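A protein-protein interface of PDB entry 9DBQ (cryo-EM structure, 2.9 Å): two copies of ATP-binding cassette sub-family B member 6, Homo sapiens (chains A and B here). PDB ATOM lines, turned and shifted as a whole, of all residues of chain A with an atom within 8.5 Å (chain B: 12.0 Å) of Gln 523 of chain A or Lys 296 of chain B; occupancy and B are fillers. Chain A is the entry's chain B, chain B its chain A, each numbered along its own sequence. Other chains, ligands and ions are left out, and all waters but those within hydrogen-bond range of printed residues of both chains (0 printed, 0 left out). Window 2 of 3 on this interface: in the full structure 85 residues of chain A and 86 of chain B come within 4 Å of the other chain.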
ATOM      1  N   CYS A 516     -16.269  -3.901   7.924  1.00  0.00           N
ATOM      2  CA  CYS A 516     -14.858  -4.025   8.276  1.00  0.00           C
ATOM      3  C   CYS A 516     -13.970  -3.803   7.059  1.00  0.00           C
ATOM      4  O   CYS A 516     -12.907  -3.183   7.165  1.00  0.00           O
ATOM      5  CB  CYS A 516     -14.594  -5.396   8.893  1.00  0.00           C
ATOM      6  SG  CYS A 516     -13.112  -5.474   9.913  1.00  0.00           S
ATOM      7  N   ALA A 517     -14.387  -4.306   5.896  1.00  0.00           N
ATOM      8  CA  ALA A 517     -13.627  -4.081   4.671  1.00  0.00           C
ATOM      9  C   ALA A 517     -13.552  -2.600   4.330  1.00  0.00           C
ATOM     10  O   ALA A 517     -12.516  -2.115   3.866  1.00  0.00           O
ATOM     11  CB  ALA A 517     -14.250  -4.862   3.518  1.00  0.00           C
ATOM     12  N   TYR A 518     -14.648  -1.867   4.525  1.00  0.00           N
ATOM     13  CA  TYR A 518     -14.624  -0.434   4.254  1.00  0.00           C
ATOM     14  C   TYR A 518     -13.676   0.293   5.193  1.00  0.00           C
ATOM     15  O   TYR A 518     -12.900   1.152   4.761  1.00  0.00           O
ATOM     16  CB  TYR A 518     -16.026   0.151   4.378  1.00  0.00           C
ATOM     17  CG  TYR A 518     -16.049   1.651   4.281  1.00  0.00           C
ATOM     18  CD1 TYR A 518     -15.778   2.287   3.085  1.00  0.00           C
ATOM     19  CD2 TYR A 518     -16.343   2.429   5.385  1.00  0.00           C
ATOM     20  CE1 TYR A 518     -15.797   3.656   2.993  1.00  0.00           C
ATOM     21  CE2 TYR A 518     -16.365   3.800   5.300  1.00  0.00           C
ATOM     22  CZ  TYR A 518     -16.092   4.408   4.102  1.00  0.00           C
ATOM     23  OH  TYR A 518     -16.113   5.780   4.011  1.00  0.00           O
ATOM     24  N   PHE A 519     -13.723  -0.032   6.486  1.00  0.00           N
ATOM     25  CA  PHE A 519     -12.905   0.698   7.447  1.00  0.00           C
ATOM     26  C   PHE A 519     -11.422   0.433   7.240  1.00  0.00           C
ATOM     27  O   PHE A 519     -10.613   1.359   7.345  1.00  0.00           O
ATOM     28  CB  PHE A 519     -13.322   0.338   8.872  1.00  0.00           C
ATOM     29  CG  PHE A 519     -14.489   1.129   9.384  1.00  0.00           C
ATOM     30  CD1 PHE A 519     -14.539   2.503   9.225  1.00  0.00           C
ATOM     31  CD2 PHE A 519     -15.536   0.499  10.027  1.00  0.00           C
ATOM     32  CE1 PHE A 519     -15.609   3.233   9.693  1.00  0.00           C
ATOM     33  CE2 PHE A 519     -16.612   1.219  10.498  1.00  0.00           C
ATOM     34  CZ  PHE A 519     -16.649   2.593  10.333  1.00  0.00           C
ATOM     35  N   VAL A 520     -11.043  -0.807   6.929  1.00  0.00           N
ATOM     36  CA  VAL A 520      -9.643  -1.085   6.637  1.00  0.00           C
ATOM     37  C   VAL A 520      -9.221  -0.457   5.318  1.00  0.00           C
ATOM     38  O   VAL A 520      -8.030  -0.203   5.112  1.00  0.00           O
ATOM     39  CB  VAL A 520      -9.377  -2.600   6.621  1.00  0.00           C
ATOM     40  CG1 VAL A 520     -10.075  -3.254   5.453  1.00  0.00           C
ATOM     41  CG2 VAL A 520      -7.889  -2.880   6.577  1.00  0.00           C
ATOM     42  N   THR A 521     -10.172  -0.203   4.417  1.00  0.00           N
ATOM     43  CA  THR A 521      -9.861   0.512   3.184  1.00  0.00           C
ATOM     44  C   THR A 521      -9.491   1.961   3.470  1.00  0.00           C
ATOM     45  O   THR A 521      -8.598   2.519   2.824  1.00  0.00           O
ATOM     46  CB  THR A 521     -11.050   0.443   2.227  1.00  0.00           C
ATOM     47  OG1 THR A 521     -11.357  -0.926   1.944  1.00  0.00           O
ATOM     48  CG2 THR A 521     -10.738   1.164   0.930  1.00  0.00           C
ATOM     49  N   GLU A 522     -10.165   2.584   4.434  1.00  0.00           N
ATOM     50  CA  GLU A 522      -9.970   3.994   4.739  1.00  0.00           C
ATOM     51  C   GLU A 522      -8.941   4.221   5.843  1.00  0.00           C
ATOM     52  O   GLU A 522      -8.963   5.273   6.491  1.00  0.00           O
ATOM     53  CB  GLU A 522     -11.302   4.634   5.119  1.00  0.00           C
ATOM     54  CG  GLU A 522     -11.375   6.110   4.785  1.00  0.00           C
ATOM     55  CD  GLU A 522     -12.746   6.694   5.033  1.00  0.00           C
ATOM     56  OE1 GLU A 522     -13.631   5.953   5.506  1.00  0.00           O
ATOM     57  OE2 GLU A 522     -12.940   7.895   4.755  1.00  0.00           O
ATOM     58  N   GLN A 523      -8.038   3.265   6.065  1.00  0.00           N
ATOM     59  CA  GLN A 523      -6.932   3.427   7.010  1.00  0.00           C
ATOM     60  C   GLN A 523      -7.432   3.737   8.419  1.00  0.00           C
ATOM     61  O   GLN A 523      -6.880   4.588   9.120  1.00  0.00           O
ATOM     62  CB  GLN A 523      -5.956   4.506   6.534  1.00  0.00           C
ATOM     63  CG  GLN A 523      -4.881   3.996   5.597  1.00  0.00           C
ATOM     64  CD  GLN A 523      -5.336   3.952   4.155  1.00  0.00           C
ATOM     65  OE1 GLN A 523      -5.717   4.971   3.580  1.00  0.00           O
ATOM     66  NE2 GLN A 523      -5.298   2.766   3.561  1.00  0.00           N
ATOM     67  N   LYS A 524      -8.494   3.052   8.838  1.00  0.00           N
ATOM     68  CA  LYS A 524      -8.988   3.147  10.206  1.00  0.00           C
ATOM     69  C   LYS A 524      -8.811   1.865  10.997  1.00  0.00           C
ATOM     70  O   LYS A 524      -8.608   1.927  12.209  1.00  0.00           O
ATOM     71  CB  LYS A 524     -10.469   3.543  10.210  1.00  0.00           C
ATOM     72  CG  LYS A 524     -10.716   4.955   9.698  1.00  0.00           C
ATOM     73  CD  LYS A 524     -12.179   5.328   9.651  1.00  0.00           C
ATOM     74  CE  LYS A 524     -12.341   6.735   9.122  1.00  0.00           C
ATOM     75  NZ  LYS A 524     -13.765   7.167   9.013  1.00  0.00           N
ATOM     76  N   LEU A 525      -8.869   0.715  10.343  1.00  0.00           N
ATOM     77  CA  LEU A 525      -8.525  -0.567  10.935  1.00  0.00           C
ATOM     78  C   LEU A 525      -7.338  -1.145  10.173  1.00  0.00           C
ATOM     79  O   LEU A 525      -6.890  -0.592   9.168  1.00  0.00           O
ATOM     80  CB  LEU A 525      -9.717  -1.526  10.909  1.00  0.00           C
ATOM     81  CG  LEU A 525     -10.898  -1.167  11.810  1.00  0.00           C
ATOM     82  CD1 LEU A 525     -11.947  -2.253  11.737  1.00  0.00           C
ATOM     83  CD2 LEU A 525     -10.456  -0.947  13.246  1.00  0.00           C
ATOM     84  N   GLN A 526      -6.821  -2.260  10.666  1.00  0.00           N
ATOM     85  CA  GLN A 526      -5.699  -2.934  10.041  1.00  0.00           C
ATOM     86  C   GLN A 526      -6.173  -4.244   9.430  1.00  0.00           C
ATOM     87  O   GLN A 526      -7.295  -4.695   9.660  1.00  0.00           O
ATOM     88  CB  GLN A 526      -4.579  -3.166  11.059  1.00  0.00           C
ATOM     89  CG  GLN A 526      -3.777  -1.915  11.355  1.00  0.00           C
ATOM     90  CD  GLN A 526      -2.819  -2.099  12.504  1.00  0.00           C
ATOM     91  OE1 GLN A 526      -3.083  -2.872  13.425  1.00  0.00           O
ATOM     92  NE2 GLN A 526      -1.696  -1.398  12.459  1.00  0.00           N
ATOM     93  N   VAL A 527      -5.298  -4.855   8.632  1.00  0.00           N
ATOM     94  CA  VAL A 527      -5.698  -6.054   7.911  1.00  0.00           C
ATOM     95  C   VAL A 527      -6.005  -7.186   8.878  1.00  0.00           C
ATOM     96  O   VAL A 527      -6.827  -8.059   8.581  1.00  0.00           O
ATOM     97  CB  VAL A 527      -4.613  -6.460   6.903  1.00  0.00           C
ATOM     98  CG1 VAL A 527      -5.107  -7.599   6.033  1.00  0.00           C
ATOM     99  CG2 VAL A 527      -4.204  -5.267   6.052  1.00  0.00           C
ATOM    100  N   ASN B 288      -8.286 -14.467  -1.619  1.00  0.00           N
ATOM    101  CA  ASN B 288      -8.366 -13.330  -2.527  1.00  0.00           C
ATOM    102  C   ASN B 288      -8.701 -12.049  -1.774  1.00  0.00           C
ATOM    103  O   ASN B 288      -8.134 -10.987  -2.055  1.00  0.00           O
ATOM    104  CB  ASN B 288      -9.404 -13.606  -3.610  1.00  0.00           C
ATOM    105  CG  ASN B 288      -8.930 -14.617  -4.622  1.00  0.00           C
ATOM    106  OD1 ASN B 288      -7.822 -15.139  -4.523  1.00  0.00           O
ATOM    107  ND2 ASN B 288      -9.771 -14.905  -5.603  1.00  0.00           N
ATOM    108  N   ILE B 289      -9.629 -12.127  -0.818  1.00  0.00           N
ATOM    109  CA  ILE B 289     -10.002 -10.950  -0.039  1.00  0.00           C
ATOM    110  C   ILE B 289      -8.797 -10.417   0.725  1.00  0.00           C
ATOM    111  O   ILE B 289      -8.503  -9.217   0.701  1.00  0.00           O
ATOM    112  CB  ILE B 289     -11.163 -11.291   0.911  1.00  0.00           C
ATOM    113  CG1 ILE B 289     -12.454 -11.475   0.117  1.00  0.00           C
ATOM    114  CG2 ILE B 289     -11.323 -10.215   1.976  1.00  0.00           C
ATOM    115  CD1 ILE B 289     -13.634 -11.881   0.959  1.00  0.00           C
ATOM    116  N   VAL B 290      -8.079 -11.306   1.412  1.00  0.00           N
ATOM    117  CA  VAL B 290      -6.951 -10.874   2.229  1.00  0.00           C
ATOM    118  C   VAL B 290      -5.846 -10.296   1.356  1.00  0.00           C
ATOM    119  O   VAL B 290      -5.236  -9.279   1.701  1.00  0.00           O
ATOM    120  CB  VAL B 290      -6.449 -12.045   3.090  1.00  0.00           C
ATOM    121  CG1 VAL B 290      -5.204 -11.653   3.856  1.00  0.00           C
ATOM    122  CG2 VAL B 290      -7.539 -12.489   4.045  1.00  0.00           C
ATOM    123  N   ASN B 291      -5.567 -10.924   0.215  1.00  0.00           N
ATOM    124  CA  ASN B 291      -4.548 -10.385  -0.677  1.00  0.00           C
ATOM    125  C   ASN B 291      -4.947  -9.026  -1.236  1.00  0.00           C
ATOM    126  O   ASN B 291      -4.074  -8.213  -1.555  1.00  0.00           O
ATOM    127  CB  ASN B 291      -4.268 -11.360  -1.819  1.00  0.00           C
ATOM    128  CG  ASN B 291      -3.465 -12.560  -1.377  1.00  0.00           C
ATOM    129  OD1 ASN B 291      -2.979 -12.616  -0.250  1.00  0.00           O
ATOM    130  ND2 ASN B 291      -3.306 -13.524  -2.271  1.00  0.00           N
ATOM    131  N   LEU B 292      -6.247  -8.765  -1.383  1.00  0.00           N
ATOM    132  CA  LEU B 292      -6.682  -7.451  -1.844  1.00  0.00           C
ATOM    133  C   LEU B 292      -6.556  -6.405  -0.742  1.00  0.00           C
ATOM    134  O   LEU B 292      -6.229  -5.246  -1.015  1.00  0.00           O
ATOM    135  CB  LEU B 292      -8.121  -7.516  -2.352  1.00  0.00           C
ATOM    136  CG  LEU B 292      -8.362  -8.121  -3.739  1.00  0.00           C
ATOM    137  CD1 LEU B 292      -9.841  -8.076  -4.077  1.00  0.00           C
ATOM    138  CD2 LEU B 292      -7.553  -7.405  -4.802  1.00  0.00           C
ATOM    139  N   LEU B 293      -6.819  -6.791   0.508  1.00  0.00           N
ATOM    140  CA  LEU B 293      -6.663  -5.851   1.614  1.00  0.00           C
ATOM    141  C   LEU B 293      -5.197  -5.511   1.850  1.00  0.00           C
ATOM    142  O   LEU B 293      -4.860  -4.353   2.112  1.00  0.00           O
ATOM    143  CB  LEU B 293      -7.279  -6.422   2.890  1.00  0.00           C
ATOM    144  CG  LEU B 293      -8.791  -6.634   2.937  1.00  0.00           C
ATOM    145  CD1 LEU B 293      -9.210  -7.112   4.316  1.00  0.00           C
ATOM    146  CD2 LEU B 293      -9.523  -5.367   2.571  1.00  0.00           C
ATOM    147  N   THR B 294      -4.310  -6.507   1.756  1.00  0.00           N
ATOM    148  CA  THR B 294      -2.899  -6.267   2.047  1.00  0.00           C
ATOM    149  C   THR B 294      -2.300  -5.246   1.091  1.00  0.00           C
ATOM    150  O   THR B 294      -1.363  -4.531   1.460  1.00  0.00           O
ATOM    151  CB  THR B 294      -2.108  -7.569   1.971  1.00  0.00           C
ATOM    152  OG1 THR B 294      -2.384  -8.224   0.727  1.00  0.00           O
ATOM    153  CG2 THR B 294      -2.481  -8.488   3.117  1.00  0.00           C
ATOM    154  N   GLU B 295      -2.815  -5.169  -0.130  1.00  0.00           N
ATOM    155  CA  GLU B 295      -2.479  -4.101  -1.053  1.00  0.00           C
ATOM    156  C   GLU B 295      -3.618  -3.086  -1.057  1.00  0.00           C
ATOM    157  O   GLU B 295      -4.657  -3.274  -0.419  1.00  0.00           O
ATOM    158  CB  GLU B 295      -2.210  -4.666  -2.449  1.00  0.00           C
ATOM    159  CG  GLU B 295      -3.402  -5.360  -3.087  1.00  0.00           C
ATOM    160  CD  GLU B 295      -2.996  -6.394  -4.121  1.00  0.00           C
ATOM    161  OE1 GLU B 295      -1.796  -6.724  -4.204  1.00  0.00           O
ATOM    162  OE2 GLU B 295      -3.882  -6.881  -4.853  1.00  0.00           O
ATOM    163  N   LYS B 296      -3.426  -1.993  -1.785  1.00  0.00           N
ATOM    164  CA  LYS B 296      -4.370  -0.876  -1.758  1.00  0.00           C
ATOM    165  C   LYS B 296      -5.390  -1.002  -2.890  1.00  0.00           C
ATOM    166  O   LYS B 296      -5.466  -0.179  -3.802  1.00  0.00           O
ATOM    167  CB  LYS B 296      -3.616   0.448  -1.833  1.00  0.00           C
ATOM    168  CG  LYS B 296      -2.512   0.582  -0.790  1.00  0.00           C
ATOM    169  CD  LYS B 296      -3.028   0.321   0.615  1.00  0.00           C
ATOM    170  CE  LYS B 296      -1.943   0.510   1.661  1.00  0.00           C
ATOM    171  NZ  LYS B 296      -2.456   0.243   3.034  1.00  0.00           N
ATOM    172  N   ALA B 297      -6.187  -2.062  -2.811  1.00  0.00           N
ATOM    173  CA  ALA B 297      -7.215  -2.286  -3.813  1.00  0.00           C
ATOM    174  C   ALA B 297      -8.379  -1.319  -3.594  1.00  0.00           C
ATOM    175  O   ALA B 297      -8.735  -1.028  -2.448  1.00  0.00           O
ATOM    176  CB  ALA B 297      -7.718  -3.725  -3.751  1.00  0.00           C
ATOM    177  N   PRO B 298      -8.997  -0.813  -4.661  1.00  0.00           N
ATOM    178  CA  PRO B 298     -10.110   0.126  -4.487  1.00  0.00           C
ATOM    179  C   PRO B 298     -11.338  -0.547  -3.891  1.00  0.00           C
ATOM    180  O   PRO B 298     -11.477  -1.771  -3.881  1.00  0.00           O
ATOM    181  CB  PRO B 298     -10.392   0.620  -5.910  1.00  0.00           C
ATOM    182  CG  PRO B 298      -9.178   0.320  -6.677  1.00  0.00           C
ATOM    183  CD  PRO B 298      -8.593  -0.910  -6.073  1.00  0.00           C
ATOM    184  N   TRP B 299     -12.242   0.296  -3.386  1.00  0.00           N
ATOM    185  CA  TRP B 299     -13.474  -0.199  -2.778  1.00  0.00           C
ATOM    186  C   TRP B 299     -14.412  -0.821  -3.807  1.00  0.00           C
ATOM    187  O   TRP B 299     -15.292  -1.609  -3.443  1.00  0.00           O
ATOM    188  CB  TRP B 299     -14.170   0.946  -2.040  1.00  0.00           C
ATOM    189  CG  TRP B 299     -15.543   0.637  -1.533  1.00  0.00           C
ATOM    190  CD1 TRP B 299     -16.708   1.219  -1.928  1.00  0.00           C
ATOM    191  CD2 TRP B 299     -15.892  -0.319  -0.528  1.00  0.00           C
ATOM    192  NE1 TRP B 299     -17.765   0.682  -1.233  1.00  0.00           N
ATOM    193  CE2 TRP B 299     -17.287  -0.266  -0.367  1.00  0.00           C
ATOM    194  CE3 TRP B 299     -15.161  -1.218   0.250  1.00  0.00           C
ATOM    195  CZ2 TRP B 299     -17.962  -1.076   0.538  1.00  0.00           C
ATOM    196  CZ3 TRP B 299     -15.836  -2.019   1.143  1.00  0.00           C
ATOM    197  CH2 TRP B 299     -17.217  -1.942   1.283  1.00  0.00           C
ATOM    198  N   ASN B 300     -14.254  -0.482  -5.088  1.00  0.00           N
ATOM    199  CA  ASN B 300     -15.192  -0.964  -6.099  1.00  0.00           C
ATOM    200  C   ASN B 300     -15.098  -2.475  -6.275  1.00  0.00           C
ATOM    201  O   ASN B 300     -16.115  -3.177  -6.246  1.00  0.00           O
ATOM    202  CB  ASN B 300     -14.930  -0.264  -7.428  1.00  0.00           C
ATOM    203  CG  ASN B 300     -14.758   1.228  -7.277  1.00  0.00           C
ATOM    204  OD1 ASN B 300     -13.812   1.813  -7.800  1.00  0.00           O
ATOM    205  ND2 ASN B 300     -15.674   1.856  -6.551  1.00  0.00           N
ATOM    206  N   SER B 301     -13.887  -2.995  -6.481  1.00  0.00           N
ATOM    207  CA  SER B 301     -13.719  -4.434  -6.652  1.00  0.00           C
ATOM    208  C   SER B 301     -13.775  -5.176  -5.328  1.00  0.00           C
ATOM    209  O   SER B 301     -14.166  -6.346  -5.292  1.00  0.00           O
ATOM    210  CB  SER B 301     -12.395  -4.731  -7.356  1.00  0.00           C
ATOM    211  OG  SER B 301     -11.298  -4.262  -6.590  1.00  0.00           O
ATOM    212  N   LEU B 302     -13.378  -4.519  -4.240  1.00  0.00           N
ATOM    213  CA  LEU B 302     -13.394  -5.167  -2.934  1.00  0.00           C
ATOM    214  C   LEU B 302     -14.817  -5.483  -2.492  1.00  0.00           C
ATOM    215  O   LEU B 302     -15.064  -6.514  -1.858  1.00  0.00           O
ATOM    216  CB  LEU B 302     -12.698  -4.272  -1.913  1.00  0.00           C
ATOM    217  CG  LEU B 302     -12.315  -4.893  -0.573  1.00  0.00           C
ATOM    218  CD1 LEU B 302     -11.273  -5.977  -0.749  1.00  0.00           C
ATOM    219  CD2 LEU B 302     -11.811  -3.810   0.362  1.00  0.00           C
ATOM    220  N   ALA B 303     -15.767  -4.601  -2.805  1.00  0.00           N
ATOM    221  CA  ALA B 303     -17.146  -4.807  -2.376  1.00  0.00           C
ATOM    222  C   ALA B 303     -17.744  -6.057  -3.009  1.00  0.00           C
ATOM    223  O   ALA B 303     -18.420  -6.843  -2.339  1.00  0.00           O
ATOM    224  CB  ALA B 303     -17.986  -3.580  -2.715  1.00  0.00           C
ATOM    225  N   THR B 305     -16.069  -8.621  -4.275  1.00  0.00           N
ATOM    226  CA  THR B 305     -15.346  -9.799  -3.807  1.00  0.00           C
ATOM    227  C   THR B 305     -15.837 -10.243  -2.435  1.00  0.00           C
ATOM    228  O   THR B 305     -15.988 -11.443  -2.182  1.00  0.00           O
ATOM    229  CB  THR B 305     -13.848  -9.508  -3.770  1.00  0.00           C
ATOM    230  OG1 THR B 305     -13.433  -8.987  -5.036  1.00  0.00           O
ATOM    231  CG2 THR B 305     -13.067 -10.774  -3.469  1.00  0.00           C
ATOM    232  N   GLN B 526       2.102 -15.607  -0.274  1.00  0.00           N
ATOM    233  CA  GLN B 526       1.505 -14.320   0.033  1.00  0.00           C
ATOM    234  C   GLN B 526       0.779 -14.406   1.366  1.00  0.00           C
ATOM    235  O   GLN B 526       0.584 -15.486   1.926  1.00  0.00           O
ATOM    236  CB  GLN B 526       0.562 -13.886  -1.091  1.00  0.00           C
ATOM    237  CG  GLN B 526       1.292 -13.360  -2.312  1.00  0.00           C
ATOM    238  CD  GLN B 526       0.376 -13.148  -3.490  1.00  0.00           C
ATOM    239  OE1 GLN B 526      -0.624 -13.848  -3.643  1.00  0.00           O
ATOM    240  NE2 GLN B 526       0.706 -12.176  -4.329  1.00  0.00           N
ATOM    241  N   VAL B 527       0.383 -13.244   1.881  1.00  0.00           N
ATOM    242  CA  VAL B 527      -0.214 -13.213   3.209  1.00  0.00           C
ATOM    243  C   VAL B 527      -1.535 -13.966   3.222  1.00  0.00           C
ATOM    244  O   VAL B 527      -1.934 -14.513   4.255  1.00  0.00           O
ATOM    245  CB  VAL B 527      -0.394 -11.763   3.682  1.00  0.00           C
ATOM    246  CG1 VAL B 527      -0.849 -11.738   5.127  1.00  0.00           C
ATOM    247  CG2 VAL B 527       0.900 -10.983   3.509  1.00  0.00           C
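2 positions are printed for both chains. Of the 7 pairs that touch across the chains among the printed residues, none has its exchanged pair printed and touching as well.
Hydrophobic or aromatic side chains of chain A that line the printed part of chain B: Tyr 518, Val 520 and Val 527. Of the 19 printed residues of chain B, 4 touch a printed residue of chain A. Hydrophobic or aromatic side chains of chain B that line the printed part of chain A: Leu 293, Trp 299 and Leu 302. Among the printed residues, 7 pairs touch across the chains.
Among the printed residues, pairs that only touch across the chains: Ala 517 of chain A with Trp 299 of chain B, Ala 517 of chain A with Leu 302 of chain B, Tyr 518 of chain A with Trp 299 of chain B, Val 520 of chain A with Leu 293 of chain B, Thr 521 of chain A with Leu 302 of chain B, Gln 523 of chain A with Lys 296 of chain B and Val 527 of chain A with Leu 293 of chain B.
Of chain B, only Lys 296 (3.8 Å) comes within 4 Å of Gln 523 of chain A. Of the printed residues of chain A, Lys 296 of chain B touches Gln 523. Of chain B, only Leu 302 (3.3 Å) comes within 4 Å of Thr 521 of chain A. Of the printed residues of chain A, Trp 299 of chain B touches Ala 517 and Tyr 518. Printed residues of chain A within 4 Å of Leu 293 of chain B: Val 520 and Val 527. Printed residues of chain B within 4 Å of Val 527 of chain A: Leu 293. Of the printed residues of chain A, Leu 302 of chain B touches Ala 517 (3.96 Å) and Thr 521 (3.3 Å). Val 290 of chain B touches none of the printed residues of chain A. Gln 526 of chain B touches none of the printed residues of chain A. The nearest printed residue of chain B that does not touch Gln 523 of chain A is Glu 295 of chain B (7.3 Å). The nearest residue of chain A that does not touch Lys 296 of chain B is Val 520 of chain A (6.0 Å). The nearest printed residue of chain A that does not touch Leu 293 of chain B is Ala 517 of chain A (4.6 Å).
The side-chain amide nitrogen (NE2) of Gln 523 of chain A lies within hydrogen-bond range of the backbone carbonyl oxygen (O) of Thr 521 of chain A, at 3.4 Å. OG1 of Thr 521 of chain A lies within hydrogen-bond range of O of Ala 517 of chain A. The side-chain hydroxyl (OH) of Tyr 518 of chain A lies within hydrogen-bond range of the side-chain carboxylate (OE1) of Glu 522 of chain A.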
